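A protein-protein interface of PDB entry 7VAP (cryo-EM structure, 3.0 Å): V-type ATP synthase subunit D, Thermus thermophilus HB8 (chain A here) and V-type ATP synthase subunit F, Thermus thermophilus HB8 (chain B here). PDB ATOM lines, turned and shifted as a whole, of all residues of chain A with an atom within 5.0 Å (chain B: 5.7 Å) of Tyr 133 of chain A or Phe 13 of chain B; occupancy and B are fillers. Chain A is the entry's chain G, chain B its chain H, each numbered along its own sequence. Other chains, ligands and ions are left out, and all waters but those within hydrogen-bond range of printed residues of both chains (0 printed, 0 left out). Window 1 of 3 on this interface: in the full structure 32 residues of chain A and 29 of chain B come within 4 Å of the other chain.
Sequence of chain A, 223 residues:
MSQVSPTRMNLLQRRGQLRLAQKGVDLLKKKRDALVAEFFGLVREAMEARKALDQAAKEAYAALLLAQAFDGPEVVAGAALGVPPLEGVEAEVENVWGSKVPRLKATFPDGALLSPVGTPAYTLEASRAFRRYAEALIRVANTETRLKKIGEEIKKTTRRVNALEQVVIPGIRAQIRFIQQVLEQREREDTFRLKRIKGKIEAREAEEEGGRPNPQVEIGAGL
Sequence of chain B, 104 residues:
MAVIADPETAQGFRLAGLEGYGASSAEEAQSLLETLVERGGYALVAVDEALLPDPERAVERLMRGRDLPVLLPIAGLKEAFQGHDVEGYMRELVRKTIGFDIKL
O of Phe 13 of chain B lies within hydrogen-bond range of N of Leu 18 of chain B, 2.8 Å away.
Gly 12 of chain B touches Phe 130 of chain A.
Phe 130 of chain A touches Ala 16 of chain B (CB to CB, 3.5 Å).
Arg 131 of chain A touches Ala 16 of chain B (CG to O, 3.5 Å).
Tyr 133 of chain A touches Phe 13 of chain B.
Tyr 133 of chain A touches Ile 74 of chain B (OH to CD1, 3.1 Å).
CD1 of Leu 18 of chain B touches CB of Ala 134 of chain A, at 3.7 Å.
CD1 of Leu 137 of chain A touches CD1 of Ile 74 of chain B (3.6 Å).
Tyr 133 of chain A touches two residues of chain B.
Phe 13 of chain B touches one residue of chain A.
Of the printed residues of chain B, Arg 131 of chain A touches Ala 16.
Of the printed residues of chain B, Ala 134 of chain A touches Leu 18 (3.7 Å).
Of the printed residues of chain A, Gly 12 of chain B touches Phe 130.
Of the printed residues of chain A, Leu 18 of chain B touches Ala 134.
The nearest residue of chain A that does not touch Phe 13 of chain B is Phe 130 of chain A (4.5 Å).
Of the 16 printed residues of chain B, 5 touch a printed residue of chain A.
Hydrophobic or aromatic side chains of chain B within 4 Å of the printed part of chain A: Phe 13, Ala 16, Leu 18 and Ile 74.
Hydrophobic or aromatic side chains of chain A that line the printed part of chain B: Phe 130, Tyr 133, Ala 134 and Leu 137.
Among the printed residues, 7 pairs touch across the chains.
Among the printed residues, no Asp or Glu carboxylate lies within 4 Å of a Lys or Arg side-chain nitrogen of the other chain.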
ATOM      1  N   LEU A  53     -20.940   4.729  23.828  1.00  0.00           N
ATOM      2  CA  LEU A  53     -20.695   3.870  22.674  1.00  0.00           C
ATOM      3  C   LEU A  53     -19.210   3.786  22.360  1.00  0.00           C
ATOM      4  O   LEU A  53     -18.702   2.715  22.012  1.00  0.00           O
ATOM      5  CB  LEU A  53     -21.466   4.389  21.462  1.00  0.00           C
ATOM      6  CG  LEU A  53     -21.119   3.754  20.115  1.00  0.00           C
ATOM      7  CD1 LEU A  53     -21.689   2.352  20.039  1.00  0.00           C
ATOM      8  CD2 LEU A  53     -21.624   4.606  18.961  1.00  0.00           C
ATOM      9  N   ALA A  56     -17.614   1.469  24.868  1.00  0.00           N
ATOM     10  CA  ALA A  56     -17.950   0.081  24.560  1.00  0.00           C
ATOM     11  C   ALA A  56     -17.157  -0.423  23.362  1.00  0.00           C
ATOM     12  O   ALA A  56     -16.682  -1.565  23.358  1.00  0.00           O
ATOM     13  CB  ALA A  56     -19.450  -0.056  24.307  1.00  0.00           C
ATOM     14  N   ALA A  57     -17.005   0.416  22.334  1.00  0.00           N
ATOM     15  CA  ALA A  57     -16.193   0.046  21.181  1.00  0.00           C
ATOM     16  C   ALA A  57     -14.751  -0.212  21.588  1.00  0.00           C
ATOM     17  O   ALA A  57     -14.134  -1.182  21.134  1.00  0.00           O
ATOM     18  CB  ALA A  57     -16.253   1.143  20.119  1.00  0.00           C
ATOM     19  N   ALA A  60     -14.585  -3.574  23.508  1.00  0.00           N
ATOM     20  CA  ALA A  60     -14.863  -4.716  22.645  1.00  0.00           C
ATOM     21  C   ALA A  60     -13.714  -4.978  21.680  1.00  0.00           C
ATOM     22  O   ALA A  60     -13.319  -6.133  21.472  1.00  0.00           O
ATOM     23  CB  ALA A  60     -16.167  -4.487  21.883  1.00  0.00           C
ATOM     24  N   ARG A 128     -19.734 -11.478  23.726  1.00  0.00           N
ATOM     25  CA  ARG A 128     -20.517 -10.683  24.669  1.00  0.00           C
ATOM     26  C   ARG A 128     -20.162  -9.204  24.577  1.00  0.00           C
ATOM     27  O   ARG A 128     -21.047  -8.338  24.626  1.00  0.00           O
ATOM     28  CB  ARG A 128     -20.296 -11.201  26.092  1.00  0.00           C
ATOM     29  CG  ARG A 128     -21.066 -10.441  27.160  1.00  0.00           C
ATOM     30  CD  ARG A 128     -22.505 -10.923  27.251  1.00  0.00           C
ATOM     31  NE  ARG A 128     -23.385 -10.189  26.350  1.00  0.00           N
ATOM     32  CZ  ARG A 128     -24.615 -10.567  26.033  1.00  0.00           C
ATOM     33  NH1 ARG A 128     -25.149 -11.670  26.531  1.00  0.00           N
ATOM     34  NH2 ARG A 128     -25.329  -9.818  25.198  1.00  0.00           N
ATOM     35  N   ALA A 129     -18.868  -8.895  24.455  1.00  0.00           N
ATOM     36  CA  ALA A 129     -18.454  -7.503  24.325  1.00  0.00           C
ATOM     37  C   ALA A 129     -19.030  -6.879  23.064  1.00  0.00           C
ATOM     38  O   ALA A 129     -19.519  -5.746  23.091  1.00  0.00           O
ATOM     39  CB  ALA A 129     -16.929  -7.404  24.327  1.00  0.00           C
ATOM     40  N   PHE A 130     -18.997  -7.614  21.951  1.00  0.00           N
ATOM     41  CA  PHE A 130     -19.573  -7.103  20.713  1.00  0.00           C
ATOM     42  C   PHE A 130     -21.081  -6.938  20.813  1.00  0.00           C
ATOM     43  O   PHE A 130     -21.636  -5.994  20.244  1.00  0.00           O
ATOM     44  CB  PHE A 130     -19.215  -8.027  19.552  1.00  0.00           C
ATOM     45  CG  PHE A 130     -17.780  -7.941  19.140  1.00  0.00           C
ATOM     46  CD1 PHE A 130     -17.003  -6.867  19.531  1.00  0.00           C
ATOM     47  CD2 PHE A 130     -17.205  -8.938  18.376  1.00  0.00           C
ATOM     48  CE1 PHE A 130     -15.685  -6.781  19.160  1.00  0.00           C
ATOM     49  CE2 PHE A 130     -15.883  -8.858  18.004  1.00  0.00           C
ATOM     50  CZ  PHE A 130     -15.124  -7.776  18.395  1.00  0.00           C
ATOM     51  N   ARG A 131     -21.761  -7.836  21.526  1.00  0.00           N
ATOM     52  CA  ARG A 131     -23.206  -7.704  21.683  1.00  0.00           C
ATOM     53  C   ARG A 131     -23.564  -6.475  22.515  1.00  0.00           C
ATOM     54  O   ARG A 131     -24.499  -5.739  22.178  1.00  0.00           O
ATOM     55  CB  ARG A 131     -23.773  -8.978  22.305  1.00  0.00           C
ATOM     56  CG  ARG A 131     -23.964 -10.104  21.297  1.00  0.00           C
ATOM     57  CD  ARG A 131     -24.426 -11.389  21.962  1.00  0.00           C
ATOM     58  NE  ARG A 131     -23.315 -12.277  22.281  1.00  0.00           N
ATOM     59  CZ  ARG A 131     -23.441 -13.429  22.926  1.00  0.00           C
ATOM     60  NH1 ARG A 131     -24.621 -13.869  23.329  1.00  0.00           N
ATOM     61  NH2 ARG A 131     -22.356 -14.156  23.173  1.00  0.00           N
ATOM     62  N   ARG A 132     -22.823  -6.230  23.598  1.00  0.00           N
ATOM     63  CA  ARG A 132     -23.055  -5.025  24.392  1.00  0.00           C
ATOM     64  C   ARG A 132     -22.700  -3.768  23.602  1.00  0.00           C
ATOM     65  O   ARG A 132     -23.360  -2.728  23.730  1.00  0.00           O
ATOM     66  CB  ARG A 132     -22.258  -5.107  25.694  1.00  0.00           C
ATOM     67  CG  ARG A 132     -22.884  -6.042  26.724  1.00  0.00           C
ATOM     68  CD  ARG A 132     -22.059  -6.130  27.995  1.00  0.00           C
ATOM     69  NE  ARG A 132     -21.005  -7.135  27.894  1.00  0.00           N
ATOM     70  CZ  ARG A 132     -19.742  -6.874  27.591  1.00  0.00           C
ATOM     71  NH1 ARG A 132     -19.333  -5.643  27.325  1.00  0.00           N
ATOM     72  NH2 ARG A 132     -18.865  -7.873  27.553  1.00  0.00           N
ATOM     73  N   TYR A 133     -21.663  -3.857  22.767  1.00  0.00           N
ATOM     74  CA  TYR A 133     -21.314  -2.764  21.868  1.00  0.00           C
ATOM     75  C   TYR A 133     -22.451  -2.474  20.895  1.00  0.00           C
ATOM     76  O   TYR A 133     -22.785  -1.311  20.640  1.00  0.00           O
ATOM     77  CB  TYR A 133     -20.027  -3.136  21.128  1.00  0.00           C
ATOM     78  CG  TYR A 133     -19.585  -2.203  20.029  1.00  0.00           C
ATOM     79  CD1 TYR A 133     -19.720  -0.829  20.152  1.00  0.00           C
ATOM     80  CD2 TYR A 133     -18.999  -2.703  18.875  1.00  0.00           C
ATOM     81  CE1 TYR A 133     -19.303   0.019  19.148  1.00  0.00           C
ATOM     82  CE2 TYR A 133     -18.576  -1.862  17.869  1.00  0.00           C
ATOM     83  CZ  TYR A 133     -18.731  -0.503  18.011  1.00  0.00           C
ATOM     84  OH  TYR A 133     -18.310   0.340  17.012  1.00  0.00           O
ATOM     85  N   ALA A 134     -23.068  -3.525  20.354  1.00  0.00           N
ATOM     86  CA  ALA A 134     -24.203  -3.348  19.456  1.00  0.00           C
ATOM     87  C   ALA A 134     -25.403  -2.764  20.189  1.00  0.00           C
ATOM     88  O   ALA A 134     -26.176  -1.994  19.609  1.00  0.00           O
ATOM     89  CB  ALA A 134     -24.565  -4.679  18.800  1.00  0.00           C
ATOM     90  N   GLU A 135     -25.589  -3.131  21.458  1.00  0.00           N
ATOM     91  CA  GLU A 135     -26.656  -2.523  22.249  1.00  0.00           C
ATOM     92  C   GLU A 135     -26.426  -1.025  22.418  1.00  0.00           C
ATOM     93  O   GLU A 135     -27.358  -0.219  22.275  1.00  0.00           O
ATOM     94  CB  GLU A 135     -26.754  -3.209  23.612  1.00  0.00           C
ATOM     95  CG  GLU A 135     -27.903  -2.718  24.478  1.00  0.00           C
ATOM     96  CD  GLU A 135     -27.510  -1.550  25.364  1.00  0.00           C
ATOM     97  OE1 GLU A 135     -26.312  -1.436  25.701  1.00  0.00           O
ATOM     98  OE2 GLU A 135     -28.397  -0.744  25.717  1.00  0.00           O
ATOM     99  N   ALA A 136     -25.186  -0.635  22.722  1.00  0.00           N
ATOM    100  CA  ALA A 136     -24.862   0.787  22.809  1.00  0.00           C
ATOM    101  C   ALA A 136     -25.086   1.478  21.470  1.00  0.00           C
ATOM    102  O   ALA A 136     -25.556   2.621  21.420  1.00  0.00           O
ATOM    103  CB  ALA A 136     -23.419   0.974  23.276  1.00  0.00           C
ATOM    104  N   LEU A 137     -24.751   0.796  20.373  1.00  0.00           N
ATOM    105  CA  LEU A 137     -24.983   1.351  19.044  1.00  0.00           C
ATOM    106  C   LEU A 137     -26.470   1.560  18.780  1.00  0.00           C
ATOM    107  O   LEU A 137     -26.868   2.577  18.199  1.00  0.00           O
ATOM    108  CB  LEU A 137     -24.374   0.430  17.988  1.00  0.00           C
ATOM    109  CG  LEU A 137     -24.295   0.988  16.571  1.00  0.00           C
ATOM    110  CD1 LEU A 137     -23.366   2.184  16.538  1.00  0.00           C
ATOM    111  CD2 LEU A 137     -23.828  -0.089  15.606  1.00  0.00           C
ATOM    112  N   VAL B   3     -23.475  -3.760   9.195  1.00  0.00           N
ATOM    113  CA  VAL B   3     -22.337  -2.858   9.331  1.00  0.00           C
ATOM    114  C   VAL B   3     -21.439  -3.020   8.113  1.00  0.00           C
ATOM    115  O   VAL B   3     -21.224  -4.139   7.635  1.00  0.00           O
ATOM    116  CB  VAL B   3     -21.536  -3.128  10.624  1.00  0.00           C
ATOM    117  CG1 VAL B   3     -20.470  -2.063  10.819  1.00  0.00           C
ATOM    118  CG2 VAL B   3     -22.454  -3.190  11.835  1.00  0.00           C
ATOM    119  N   ALA B   5     -17.549  -1.996   7.322  1.00  0.00           N
ATOM    120  CA  ALA B   5     -16.350  -1.554   8.031  1.00  0.00           C
ATOM    121  C   ALA B   5     -15.207  -2.491   7.654  1.00  0.00           C
ATOM    122  O   ALA B   5     -15.313  -3.274   6.701  1.00  0.00           O
ATOM    123  CB  ALA B   5     -16.587  -1.506   9.541  1.00  0.00           C
ATOM    124  N   THR B   9     -13.134  -6.126  11.924  1.00  0.00           N
ATOM    125  CA  THR B   9     -14.329  -5.923  12.731  1.00  0.00           C
ATOM    126  C   THR B   9     -15.592  -6.436  12.054  1.00  0.00           C
ATOM    127  O   THR B   9     -16.600  -6.642  12.736  1.00  0.00           O
ATOM    128  CB  THR B   9     -14.496  -4.441  13.079  1.00  0.00           C
ATOM    129  OG1 THR B   9     -15.520  -4.292  14.071  1.00  0.00           O
ATOM    130  CG2 THR B   9     -14.869  -3.638  11.849  1.00  0.00           C
ATOM    131  N   ALA B  10     -15.564  -6.654  10.737  1.00  0.00           N
ATOM    132  CA  ALA B  10     -16.719  -7.246  10.069  1.00  0.00           C
ATOM    133  C   ALA B  10     -16.939  -8.681  10.534  1.00  0.00           C
ATOM    134  O   ALA B  10     -18.066  -9.077  10.859  1.00  0.00           O
ATOM    135  CB  ALA B  10     -16.534  -7.186   8.552  1.00  0.00           C
ATOM    136  N   GLN B  11     -15.865  -9.472  10.586  1.00  0.00           N
ATOM    137  CA  GLN B  11     -15.980 -10.818  11.130  1.00  0.00           C
ATOM    138  C   GLN B  11     -16.319 -10.786  12.613  1.00  0.00           C
ATOM    139  O   GLN B  11     -16.989 -11.693  13.116  1.00  0.00           O
ATOM    140  CB  GLN B  11     -14.691 -11.603  10.882  1.00  0.00           C
ATOM    141  CG  GLN B  11     -13.461 -11.034  11.564  1.00  0.00           C
ATOM    142  CD  GLN B  11     -12.190 -11.753  11.159  1.00  0.00           C
ATOM    143  OE1 GLN B  11     -12.202 -12.599  10.265  1.00  0.00           O
ATOM    144  NE2 GLN B  11     -11.087 -11.421  11.815  1.00  0.00           N
ATOM    145  N   GLY B  12     -15.894  -9.742  13.325  1.00  0.00           N
ATOM    146  CA  GLY B  12     -16.300  -9.602  14.713  1.00  0.00           C
ATOM    147  C   GLY B  12     -17.794  -9.384  14.863  1.00  0.00           C
ATOM    148  O   GLY B  12     -18.435  -9.979  15.734  1.00  0.00           O
ATOM    149  N   PHE B  13     -18.370  -8.533  14.012  1.00  0.00           N
ATOM    150  CA  PHE B  13     -19.814  -8.323  14.045  1.00  0.00           C
ATOM    151  C   PHE B  13     -20.558  -9.584  13.629  1.00  0.00           C
ATOM    152  O   PHE B  13     -21.642  -9.873  14.150  1.00  0.00           O
ATOM    153  CB  PHE B  13     -20.198  -7.144  13.153  1.00  0.00           C
ATOM    154  CG  PHE B  13     -19.789  -5.810  13.705  1.00  0.00           C
ATOM    155  CD1 PHE B  13     -20.094  -5.466  15.011  1.00  0.00           C
ATOM    156  CD2 PHE B  13     -19.109  -4.897  12.919  1.00  0.00           C
ATOM    157  CE1 PHE B  13     -19.721  -4.239  15.525  1.00  0.00           C
ATOM    158  CE2 PHE B  13     -18.731  -3.669  13.428  1.00  0.00           C
ATOM    159  CZ  PHE B  13     -19.039  -3.339  14.732  1.00  0.00           C
ATOM    160  N   ARG B  14     -19.996 -10.344  12.688  1.00  0.00           N
ATOM    161  CA  ARG B  14     -20.580 -11.642  12.360  1.00  0.00           C
ATOM    162  C   ARG B  14     -20.534 -12.581  13.560  1.00  0.00           C
ATOM    163  O   ARG B  14     -21.475 -13.346  13.798  1.00  0.00           O
ATOM    164  CB  ARG B  14     -19.863 -12.260  11.160  1.00  0.00           C
ATOM    165  CG  ARG B  14     -20.397 -13.628  10.767  1.00  0.00           C
ATOM    166  CD  ARG B  14     -21.881 -13.569  10.426  1.00  0.00           C
ATOM    167  NE  ARG B  14     -22.146 -12.876   9.172  1.00  0.00           N
ATOM    168  CZ  ARG B  14     -21.940 -13.396   7.969  1.00  0.00           C
ATOM    169  NH1 ARG B  14     -21.466 -14.622   7.819  1.00  0.00           N
ATOM    170  NH2 ARG B  14     -22.222 -12.670   6.891  1.00  0.00           N
ATOM    171  N   LEU B  15     -19.441 -12.535  14.327  1.00  0.00           N
ATOM    172  CA  LEU B  15     -19.345 -13.323  15.553  1.00  0.00           C
ATOM    173  C   LEU B  15     -20.386 -12.896  16.578  1.00  0.00           C
ATOM    174  O   LEU B  15     -20.918 -13.737  17.311  1.00  0.00           O
ATOM    175  CB  LEU B  15     -17.940 -13.200  16.146  1.00  0.00           C
ATOM    176  CG  LEU B  15     -17.776 -13.659  17.596  1.00  0.00           C
ATOM    177  CD1 LEU B  15     -17.843 -15.177  17.687  1.00  0.00           C
ATOM    178  CD2 LEU B  15     -16.477 -13.135  18.188  1.00  0.00           C
ATOM    179  N   ALA B  16     -20.690 -11.600  16.645  1.00  0.00           N
ATOM    180  CA  ALA B  16     -21.699 -11.115  17.578  1.00  0.00           C
ATOM    181  C   ALA B  16     -23.103 -11.592  17.233  1.00  0.00           C
ATOM    182  O   ALA B  16     -24.009 -11.441  18.059  1.00  0.00           O
ATOM    183  CB  ALA B  16     -21.685  -9.589  17.624  1.00  0.00           C
ATOM    184  N   GLY B  17     -23.303 -12.164  16.051  1.00  0.00           N
ATOM    185  CA  GLY B  17     -24.625 -12.477  15.563  1.00  0.00           C
ATOM    186  C   GLY B  17     -25.190 -11.466  14.599  1.00  0.00           C
ATOM    187  O   GLY B  17     -26.367 -11.567  14.239  1.00  0.00           O
ATOM    188  N   LEU B  18     -24.389 -10.501  14.166  1.00  0.00           N
ATOM    189  CA  LEU B  18     -24.837  -9.402  13.331  1.00  0.00           C
ATOM    190  C   LEU B  18     -24.426  -9.671  11.887  1.00  0.00           C
ATOM    191  O   LEU B  18     -23.808 -10.690  11.568  1.00  0.00           O
ATOM    192  CB  LEU B  18     -24.245  -8.084  13.834  1.00  0.00           C
ATOM    193  CG  LEU B  18     -24.520  -7.708  15.295  1.00  0.00           C
ATOM    194  CD1 LEU B  18     -23.827  -6.396  15.640  1.00  0.00           C
ATOM    195  CD2 LEU B  18     -26.006  -7.656  15.629  1.00  0.00           C
ATOM    196  N   GLU B  19     -24.768  -8.736  11.008  1.00  0.00           N
ATOM    197  CA  GLU B  19     -24.344  -8.791   9.618  1.00  0.00           C
ATOM    198  C   GLU B  19     -23.248  -7.763   9.378  1.00  0.00           C
ATOM    199  O   GLU B  19     -23.355  -6.610   9.809  1.00  0.00           O
ATOM    200  CB  GLU B  19     -25.520  -8.538   8.670  1.00  0.00           C
ATOM    201  CG  GLU B  19     -25.188  -8.696   7.188  1.00  0.00           C
ATOM    202  CD  GLU B  19     -24.849 -10.124   6.802  1.00  0.00           C
ATOM    203  OE1 GLU B  19     -23.713 -10.570   7.071  1.00  0.00           O
ATOM    204  OE2 GLU B  19     -25.722 -10.806   6.224  1.00  0.00           O
ATOM    205  N   GLY B  20     -22.187  -8.188   8.698  1.00  0.00           N
ATOM    206  CA  GLY B  20     -21.083  -7.298   8.410  1.00  0.00           C
ATOM    207  C   GLY B  20     -20.283  -7.704   7.192  1.00  0.00           C
ATOM    208  O   GLY B  20     -20.060  -8.894   6.953  1.00  0.00           O
ATOM    209  N   ILE B  74     -20.254   5.582  12.455  1.00  0.00           N
ATOM    210  CA  ILE B  74     -19.688   4.888  13.606  1.00  0.00           C
ATOM    211  C   ILE B  74     -18.201   5.198  13.694  1.00  0.00           C
ATOM    212  O   ILE B  74     -17.560   5.528  12.687  1.00  0.00           O
ATOM    213  CB  ILE B  74     -19.946   3.371  13.508  1.00  0.00           C
ATOM    214  CG1 ILE B  74     -19.874   2.711  14.884  1.00  0.00           C
ATOM    215  CG2 ILE B  74     -18.957   2.710  12.562  1.00  0.00           C
ATOM    216  CD1 ILE B  74     -20.354   1.279  14.873  1.00  0.00           C
ATOM    217  N   ALA B  75     -17.654   5.112  14.904  1.00  0.00           N
ATOM    218  CA  ALA B  75     -16.242   5.402  15.113  1.00  0.00           C
ATOM    219  C   ALA B  75     -15.372   4.293  14.533  1.00  0.00           C
ATOM    220  O   ALA B  75     -15.662   3.104  14.694  1.00  0.00           O
ATOM    221  CB  ALA B  75     -15.949   5.577  16.602  1.00  0.00           C
